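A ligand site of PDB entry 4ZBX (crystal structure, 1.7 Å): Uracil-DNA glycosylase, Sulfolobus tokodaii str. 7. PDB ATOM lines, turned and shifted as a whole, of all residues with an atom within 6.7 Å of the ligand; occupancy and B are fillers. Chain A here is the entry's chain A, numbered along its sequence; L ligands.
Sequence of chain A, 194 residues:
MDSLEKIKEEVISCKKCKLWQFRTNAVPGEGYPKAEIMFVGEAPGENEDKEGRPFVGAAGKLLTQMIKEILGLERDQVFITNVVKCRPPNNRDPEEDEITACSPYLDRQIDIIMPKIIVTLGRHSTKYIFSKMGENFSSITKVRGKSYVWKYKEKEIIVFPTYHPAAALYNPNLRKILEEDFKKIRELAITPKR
S4 of the ligand lies close to N of Cys 17, at 3.7 Å. SG of Cys 102 is bound to FE4 of the ligand (2.4 Å). An iron atom (FE1) of the ligand is bound by the side-chain sulfur of Cys 17. The backbone NH of Cys 86 sits close to a sulfur (S2) of the ligand. An iron atom (FE3) of the ligand is bound by the side-chain sulfur of Cys 86 (2.5 Å). S3 of the ligand sits close to N of Cys 102, 3.7 Å away. SG of Cys 14 is bound to FE2 of the ligand (2.4 Å).
The backbone NH of Lys 85 lies close to the side-chain sulfur of Cys 102. NZ of Lys 16 is in salt-bridge range of OE1 of Glu 10 (3.8 Å). The side-chain sulfur of Cys 17 lies close to the backbone NH of Leu 19. SG of Cys 14 lies close to N of Lys 16 (3.4 Å). OH of Tyr 105 sits at hydrogen-bond distance from NZ of Lys 16, 2.9 Å away. O of Cys 14 lies within hydrogen-bond range of NH1 of Arg 23 (2.8 Å). The guanidinium group (NH1) of Arg 23 lies close to the side-chain sulfur (SG) of Cys 86 (3.6 Å). The side-chain hydroxyl (OH) of Tyr 105 sits close to the side-chain sulfur (SG) of Cys 14.
Lys 16 touches the ligand (N to S4, 3.9 Å). CD1 of Leu 19 touches S2 of the ligand, 3.9 Å away. Trp 20 touches the ligand (CB to S4, 3.7 Å). NH1 of Arg 23 touches FE3 of the ligand (3.9 Å). Val 84 touches the ligand. Ala 101 touches the ligand. CE1 of Tyr 105 touches S1 of the ligand, 3.9 Å away. Hydrophobic or aromatic side chains that line the ligand: Leu 19, Trp 20, Val 84, Ala 101 and Tyr 105. Along chain A the residues within 4 Å of the ligand span positions 14 to 105. The nearest printed residue that does not touch the ligand is Lys 85 (4.05 Å).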
ATOM      1  N   GLU A  10      15.117  21.599  30.467  1.00  0.00           N
ATOM      2  CA  GLU A  10      13.693  21.479  30.235  1.00  0.00           C
ATOM      3  C   GLU A  10      13.360  20.081  29.728  1.00  0.00           C
ATOM      4  O   GLU A  10      12.408  19.473  30.202  1.00  0.00           O
ATOM      5  CB  GLU A  10      13.203  22.533  29.249  1.00  0.00           C
ATOM      6  CG  GLU A  10      13.182  23.932  29.829  1.00  0.00           C
ATOM      7  CD  GLU A  10      12.643  24.974  28.858  1.00  0.00           C
ATOM      8  OE1 GLU A  10      11.830  24.609  27.980  1.00  0.00           O
ATOM      9  OE2 GLU A  10      13.025  26.156  28.988  1.00  0.00           O
ATOM     10  N   VAL A  11      14.145  19.586  28.789  1.00  0.00           N
ATOM     11  CA  VAL A  11      13.879  18.274  28.201  1.00  0.00           C
ATOM     12  C   VAL A  11      13.980  17.152  29.239  1.00  0.00           C
ATOM     13  O   VAL A  11      13.132  16.253  29.298  1.00  0.00           O
ATOM     14  CB  VAL A  11      14.839  17.993  27.044  1.00  0.00           C
ATOM     15  CG1 VAL A  11      14.825  16.500  26.662  1.00  0.00           C
ATOM     16  CG2 VAL A  11      14.459  18.856  25.842  1.00  0.00           C
ATOM     17  N   ILE A  12      15.006  17.226  30.086  1.00  0.00           N
ATOM     18  CA  ILE A  12      15.298  16.140  31.026  1.00  0.00           C
ATOM     19  C   ILE A  12      14.180  15.963  32.042  1.00  0.00           C
ATOM     20  O   ILE A  12      13.909  14.850  32.522  1.00  0.00           O
ATOM     21  CB  ILE A  12      16.647  16.372  31.712  1.00  0.00           C
ATOM     22  CG1 ILE A  12      17.781  16.013  30.744  1.00  0.00           C
ATOM     23  CG2 ILE A  12      16.776  15.610  33.020  1.00  0.00           C
ATOM     24  CD1 ILE A  12      19.152  16.376  31.277  1.00  0.00           C
ATOM     25  N   SER A  13      13.463  17.044  32.322  1.00  0.00           N
ATOM     26  CA  SER A  13      12.330  16.960  33.236  1.00  0.00           C
ATOM     27  C   SER A  13      10.974  17.134  32.551  1.00  0.00           C
ATOM     28  O   SER A  13       9.965  17.319  33.224  1.00  0.00           O
ATOM     29  CB  SER A  13      12.464  18.024  34.326  1.00  0.00           C
ATOM     30  OG  SER A  13      13.524  17.699  35.202  1.00  0.00           O
ATOM     31  N   CYS A  14      10.972  17.083  31.223  1.00  0.00           N
ATOM     32  CA  CYS A  14       9.781  17.425  30.459  1.00  0.00           C
ATOM     33  C   CYS A  14       8.645  16.428  30.635  1.00  0.00           C
ATOM     34  O   CYS A  14       8.880  15.214  30.640  1.00  0.00           O
ATOM     35  CB  CYS A  14      10.126  17.510  28.971  1.00  0.00           C
ATOM     36  SG  CYS A  14       8.771  18.124  27.993  1.00  0.00           S
ATOM     37  N   LYS A  15       7.420  16.925  30.783  1.00  0.00           N
ATOM     38  CA  LYS A  15       6.258  16.053  30.783  1.00  0.00           C
ATOM     39  C   LYS A  15       5.172  16.635  29.871  1.00  0.00           C
ATOM     40  O   LYS A  15       3.989  16.510  30.153  1.00  0.00           O
ATOM     41  CB  LYS A  15       5.727  15.837  32.205  1.00  0.00           C
ATOM     42  CG  LYS A  15       6.768  15.221  33.125  1.00  0.00           C
ATOM     43  CD  LYS A  15       6.234  14.897  34.514  1.00  0.00           C
ATOM     44  CE  LYS A  15       7.352  14.320  35.369  1.00  0.00           C
ATOM     45  NZ  LYS A  15       6.908  13.969  36.751  1.00  0.00           N
ATOM     46  N   LYS A  16       5.608  17.253  28.774  1.00  0.00           N
ATOM     47  CA  LYS A  16       4.712  17.976  27.867  1.00  0.00           C
ATOM     48  C   LYS A  16       3.936  17.082  26.908  1.00  0.00           C
ATOM     49  O   LYS A  16       2.938  17.533  26.334  1.00  0.00           O
ATOM     50  CB  LYS A  16       5.499  19.012  27.070  1.00  0.00           C
ATOM     51  CG  LYS A  16       5.924  20.224  27.862  1.00  0.00           C
ATOM     52  CD  LYS A  16       6.849  21.096  27.030  1.00  0.00           C
ATOM     53  CE  LYS A  16       7.406  22.251  27.830  1.00  0.00           C
ATOM     54  NZ  LYS A  16       8.481  22.962  27.082  1.00  0.00           N
ATOM     55  N   CYS A  17       4.361  15.836  26.723  1.00  0.00           N
ATOM     56  CA  CYS A  17       3.518  14.887  25.974  1.00  0.00           C
ATOM     57  C   CYS A  17       3.529  13.515  26.637  1.00  0.00           C
ATOM     58  O   CYS A  17       4.290  13.282  27.580  1.00  0.00           O
ATOM     59  CB  CYS A  17       3.954  14.801  24.513  1.00  0.00           C
ATOM     60  SG  CYS A  17       5.334  13.680  24.149  1.00  0.00           S
ATOM     61  N   LYS A  18       2.675  12.594  26.184  1.00  0.00           N
ATOM     62  CA  LYS A  18       2.517  11.328  26.902  1.00  0.00           C
ATOM     63  C   LYS A  18       3.751  10.431  26.845  1.00  0.00           C
ATOM     64  O   LYS A  18       3.826   9.431  27.560  1.00  0.00           O
ATOM     65  CB  LYS A  18       1.289  10.559  26.388  1.00  0.00           C
ATOM     66  CG  LYS A  18       1.329  10.192  24.914  1.00  0.00           C
ATOM     67  CD  LYS A  18       0.013   9.542  24.468  1.00  0.00           C
ATOM     68  CE  LYS A  18       0.035   9.247  22.972  1.00  0.00           C
ATOM     69  NZ  LYS A  18       0.530  10.412  22.164  1.00  0.00           N
ATOM     70  N   LEU A  19       4.745  10.782  26.023  1.00  0.00           N
ATOM     71  CA  LEU A  19       5.924   9.934  25.921  1.00  0.00           C
ATOM     72  C   LEU A  19       6.745   9.920  27.212  1.00  0.00           C
ATOM     73  O   LEU A  19       7.494   8.974  27.477  1.00  0.00           O
ATOM     74  CB  LEU A  19       6.807  10.368  24.750  1.00  0.00           C
ATOM     75  CG  LEU A  19       6.221  10.151  23.365  1.00  0.00           C
ATOM     76  CD1 LEU A  19       7.233  10.462  22.281  1.00  0.00           C
ATOM     77  CD2 LEU A  19       5.669   8.728  23.199  1.00  0.00           C
ATOM     78  N   TRP A  20       6.575  10.945  28.038  1.00  0.00           N
ATOM     79  CA  TRP A  20       7.392  11.024  29.246  1.00  0.00           C
ATOM     80  C   TRP A  20       7.249   9.789  30.142  1.00  0.00           C
ATOM     81  O   TRP A  20       8.215   9.364  30.773  1.00  0.00           O
ATOM     82  CB  TRP A  20       7.071  12.305  30.034  1.00  0.00           C
ATOM     83  CG  TRP A  20       5.873  12.172  30.920  1.00  0.00           C
ATOM     84  CD1 TRP A  20       4.587  12.449  30.590  1.00  0.00           C
ATOM     85  CD2 TRP A  20       5.857  11.715  32.270  1.00  0.00           C
ATOM     86  NE1 TRP A  20       3.757  12.190  31.661  1.00  0.00           N
ATOM     87  CE2 TRP A  20       4.523  11.747  32.705  1.00  0.00           C
ATOM     88  CE3 TRP A  20       6.841  11.288  33.163  1.00  0.00           C
ATOM     89  CZ2 TRP A  20       4.152  11.358  33.990  1.00  0.00           C
ATOM     90  CZ3 TRP A  20       6.474  10.902  34.424  1.00  0.00           C
ATOM     91  CH2 TRP A  20       5.140  10.950  34.833  1.00  0.00           C
ATOM     92  N   GLN A  21       6.062   9.187  30.163  1.00  0.00           N
ATOM     93  CA  GLN A  21       5.779   8.085  31.065  1.00  0.00           C
ATOM     94  C   GLN A  21       6.528   6.800  30.716  1.00  0.00           C
ATOM     95  O   GLN A  21       6.584   5.887  31.537  1.00  0.00           O
ATOM     96  CB  GLN A  21       4.276   7.797  31.059  1.00  0.00           C
ATOM     97  CG  GLN A  21       3.791   7.190  29.751  1.00  0.00           C
ATOM     98  CD  GLN A  21       2.275   7.025  29.672  1.00  0.00           C
ATOM     99  OE1 GLN A  21       1.685   6.151  30.323  1.00  0.00           O
ATOM    100  NE2 GLN A  21       1.639   7.862  28.855  1.00  0.00           N
ATOM    101  N   ARG A  23       9.814   6.639  29.502  1.00  0.00           N
ATOM    102  CA  ARG A  23      11.256   6.821  29.326  1.00  0.00           C
ATOM    103  C   ARG A  23      12.074   6.434  30.543  1.00  0.00           C
ATOM    104  O   ARG A  23      11.571   6.447  31.680  1.00  0.00           O
ATOM    105  CB  ARG A  23      11.578   8.276  28.951  1.00  0.00           C
ATOM    106  CG  ARG A  23      11.533   9.226  30.138  1.00  0.00           C
ATOM    107  CD  ARG A  23      11.753  10.674  29.705  1.00  0.00           C
ATOM    108  NE  ARG A  23      11.552  11.553  30.853  1.00  0.00           N
ATOM    109  CZ  ARG A  23      10.943  12.726  30.801  1.00  0.00           C
ATOM    110  NH1 ARG A  23      10.467  13.177  29.640  1.00  0.00           N
ATOM    111  NH2 ARG A  23      10.787  13.442  31.909  1.00  0.00           N
ATOM    112  N   ALA A  26      15.185  11.136  29.029  1.00  0.00           N
ATOM    113  CA  ALA A  26      14.971  11.930  27.836  1.00  0.00           C
ATOM    114  C   ALA A  26      16.316  12.138  27.147  1.00  0.00           C
ATOM    115  O   ALA A  26      17.378  12.032  27.791  1.00  0.00           O
ATOM    116  CB  ALA A  26      14.315  13.260  28.163  1.00  0.00           C
ATOM    117  N   VAL A  27      16.280  12.473  25.863  1.00  0.00           N
ATOM    118  CA  VAL A  27      17.504  12.630  25.082  1.00  0.00           C
ATOM    119  C   VAL A  27      17.578  14.014  24.461  1.00  0.00           C
ATOM    120  O   VAL A  27      17.085  14.211  23.337  1.00  0.00           O
ATOM    121  CB  VAL A  27      17.588  11.555  23.989  1.00  0.00           C
ATOM    122  CG1 VAL A  27      18.939  11.627  23.257  1.00  0.00           C
ATOM    123  CG2 VAL A  27      17.393  10.148  24.600  1.00  0.00           C
ATOM    124  N   VAL A  83      14.147  14.733  16.408  1.00  0.00           N
ATOM    125  CA  VAL A  83      12.987  15.595  16.314  1.00  0.00           C
ATOM    126  C   VAL A  83      12.069  15.374  17.534  1.00  0.00           C
ATOM    127  O   VAL A  83      11.477  16.319  18.044  1.00  0.00           O
ATOM    128  CB  VAL A  83      12.254  15.364  14.963  1.00  0.00           C
ATOM    129  CG1 VAL A  83      11.749  13.919  14.836  1.00  0.00           C
ATOM    130  CG2 VAL A  83      11.127  16.363  14.799  1.00  0.00           C
ATOM    131  N   VAL A  84      12.019  14.140  18.020  1.00  0.00           N
ATOM    132  CA  VAL A  84      11.285  13.824  19.243  1.00  0.00           C
ATOM    133  C   VAL A  84      12.326  13.271  20.210  1.00  0.00           C
ATOM    134  O   VAL A  84      13.199  12.517  19.800  1.00  0.00           O
ATOM    135  CB  VAL A  84      10.151  12.825  18.987  1.00  0.00           C
ATOM    136  CG1 VAL A  84       9.633  12.215  20.293  1.00  0.00           C
ATOM    137  CG2 VAL A  84       9.021  13.509  18.216  1.00  0.00           C
ATOM    138  N   LYS A  85      12.273  13.661  21.471  1.00  0.00           N
ATOM    139  CA  LYS A  85      13.405  13.414  22.363  1.00  0.00           C
ATOM    140  C   LYS A  85      13.175  12.324  23.411  1.00  0.00           C
ATOM    141  O   LYS A  85      14.024  12.110  24.289  1.00  0.00           O
ATOM    142  CB  LYS A  85      13.801  14.727  23.013  1.00  0.00           C
ATOM    143  CG  LYS A  85      14.429  15.655  21.953  1.00  0.00           C
ATOM    144  CD  LYS A  85      14.449  17.091  22.412  1.00  0.00           C
ATOM    145  CE  LYS A  85      15.525  17.878  21.667  1.00  0.00           C
ATOM    146  NZ  LYS A  85      15.327  17.988  20.179  1.00  0.00           N
ATOM    147  N   CYS A  86      12.063  11.610  23.309  1.00  0.00           N
ATOM    148  CA  CYS A  86      11.827  10.459  24.167  1.00  0.00           C
ATOM    149  C   CYS A  86      11.419   9.258  23.333  1.00  0.00           C
ATOM    150  O   CYS A  86      10.801   9.405  22.288  1.00  0.00           O
ATOM    151  CB  CYS A  86      10.742  10.749  25.201  1.00  0.00           C
ATOM    152  SG  CYS A  86      11.313  11.992  26.364  1.00  0.00           S
ATOM    153  N   ARG A  87      11.796   8.076  23.781  1.00  0.00           N
ATOM    154  CA  ARG A  87      11.517   6.859  23.037  1.00  0.00           C
ATOM    155  C   ARG A  87      10.028   6.528  23.023  1.00  0.00           C
ATOM    156  O   ARG A  87       9.439   6.322  24.075  1.00  0.00           O
ATOM    157  CB  ARG A  87      12.322   5.706  23.639  1.00  0.00           C
ATOM    158  CG  ARG A  87      12.160   4.365  22.962  1.00  0.00           C
ATOM    159  CD  ARG A  87      12.785   3.268  23.812  1.00  0.00           C
ATOM    160  NE  ARG A  87      12.451   1.947  23.277  1.00  0.00           N
ATOM    161  CZ  ARG A  87      11.812   1.004  23.960  1.00  0.00           C
ATOM    162  NH1 ARG A  87      11.428   1.218  25.218  1.00  0.00           N
ATOM    163  NH2 ARG A  87      11.554  -0.158  23.390  1.00  0.00           N
ATOM    164  N   GLU A  98       2.877  14.326  19.382  1.00  0.00           N
ATOM    165  CA  GLU A  98       4.150  14.222  20.090  1.00  0.00           C
ATOM    166  C   GLU A  98       5.201  15.056  19.381  1.00  0.00           C
ATOM    167  O   GLU A  98       5.987  15.766  20.022  1.00  0.00           O
ATOM    168  CB  GLU A  98       4.570  12.754  20.191  1.00  0.00           C
ATOM    169  CG  GLU A  98       3.662  11.971  21.131  1.00  0.00           C
ATOM    170  CD  GLU A  98       3.648  10.470  20.869  1.00  0.00           C
ATOM    171  OE1 GLU A  98       4.447   9.982  20.043  1.00  0.00           O
ATOM    172  OE2 GLU A  98       2.825   9.796  21.514  1.00  0.00           O
ATOM    173  N   THR A 100       4.435  17.654  17.615  1.00  0.00           N
ATOM    174  CA  THR A 100       3.991  19.013  17.889  1.00  0.00           C
ATOM    175  C   THR A 100       4.481  19.484  19.254  1.00  0.00           C
ATOM    176  O   THR A 100       4.946  20.618  19.396  1.00  0.00           O
ATOM    177  CB  THR A 100       2.442  19.114  17.825  1.00  0.00           C
ATOM    178  OG1 THR A 100       2.025  18.888  16.478  1.00  0.00           O
ATOM    179  CG2 THR A 100       1.967  20.490  18.275  1.00  0.00           C
ATOM    180  N   ALA A 101       4.400  18.598  20.237  1.00  0.00           N
ATOM    181  CA  ALA A 101       4.809  18.930  21.597  1.00  0.00           C
ATOM    182  C   ALA A 101       6.322  19.112  21.720  1.00  0.00           C
ATOM    183  O   ALA A 101       6.776  20.013  22.410  1.00  0.00           O
ATOM    184  CB  ALA A 101       4.361  17.854  22.564  1.00  0.00           C
ATOM    185  N   CYS A 102       7.076  18.233  21.060  1.00  0.00           N
ATOM    186  CA  CYS A 102       8.524  18.190  21.244  1.00  0.00           C
ATOM    187  C   CYS A 102       9.312  19.072  20.270  1.00  0.00           C
ATOM    188  O   CYS A 102      10.368  19.608  20.627  1.00  0.00           O
ATOM    189  CB  CYS A 102       9.035  16.759  21.098  1.00  0.00           C
ATOM    190  SG  CYS A 102      10.612  16.508  21.947  1.00  0.00           S
ATOM    191  N   SER A 103       8.829  19.202  19.042  1.00  0.00           N
ATOM    192  CA  SER A 103       9.633  19.901  18.041  1.00  0.00           C
ATOM    193  C   SER A 103      10.031  21.350  18.392  1.00  0.00           C
ATOM    194  O   SER A 103      11.061  21.793  17.887  1.00  0.00           O
ATOM    195  CB  SER A 103       8.913  19.890  16.677  1.00  0.00           C
ATOM    196  OG  SER A 103       7.634  20.479  16.737  1.00  0.00           O
ATOM    197  N   TYR A 105      11.511  22.265  20.876  1.00  0.00           N
ATOM    198  CA  TYR A 105      12.867  22.116  21.413  1.00  0.00           C
ATOM    199  C   TYR A 105      13.867  22.130  20.268  1.00  0.00           C
ATOM    200  O   TYR A 105      14.876  22.811  20.330  1.00  0.00           O
ATOM    201  CB  TYR A 105      13.021  20.826  22.207  1.00  0.00           C
ATOM    202  CG  TYR A 105      12.303  20.807  23.550  1.00  0.00           C
ATOM    203  CD1 TYR A 105      11.499  19.729  23.927  1.00  0.00           C
ATOM    204  CD2 TYR A 105      12.468  21.855  24.463  1.00  0.00           C
ATOM    205  CE1 TYR A 105      10.858  19.706  25.150  1.00  0.00           C
ATOM    206  CE2 TYR A 105      11.827  21.841  25.697  1.00  0.00           C
ATOM    207  CZ  TYR A 105      11.043  20.761  26.035  1.00  0.00           C
ATOM    208  OH  TYR A 105      10.415  20.764  27.260  1.00  0.00           O
HETATM  209 FE1  LIG L   1       7.310  14.700  24.905  1.00  0.00          FE
HETATM  210 FE2  LIG L   1       8.742  16.381  26.415  1.00  0.00          FE
HETATM  211 FE3  LIG L   1       9.683  13.891  25.936  1.00  0.00          FE
HETATM  212 FE4  LIG L   1       9.615  15.713  23.963  1.00  0.00          FE
HETATM  213  S1  LIG L   1      10.882  15.827  25.813  1.00  0.00           S
HETATM  214  S2  LIG L   1       8.962  13.558  23.800  1.00  0.00           S
HETATM  215  S3  LIG L   1       7.705  16.860  24.475  1.00  0.00           S
HETATM  216  S4  LIG L   1       7.785  14.453  27.109  1.00  0.00           S
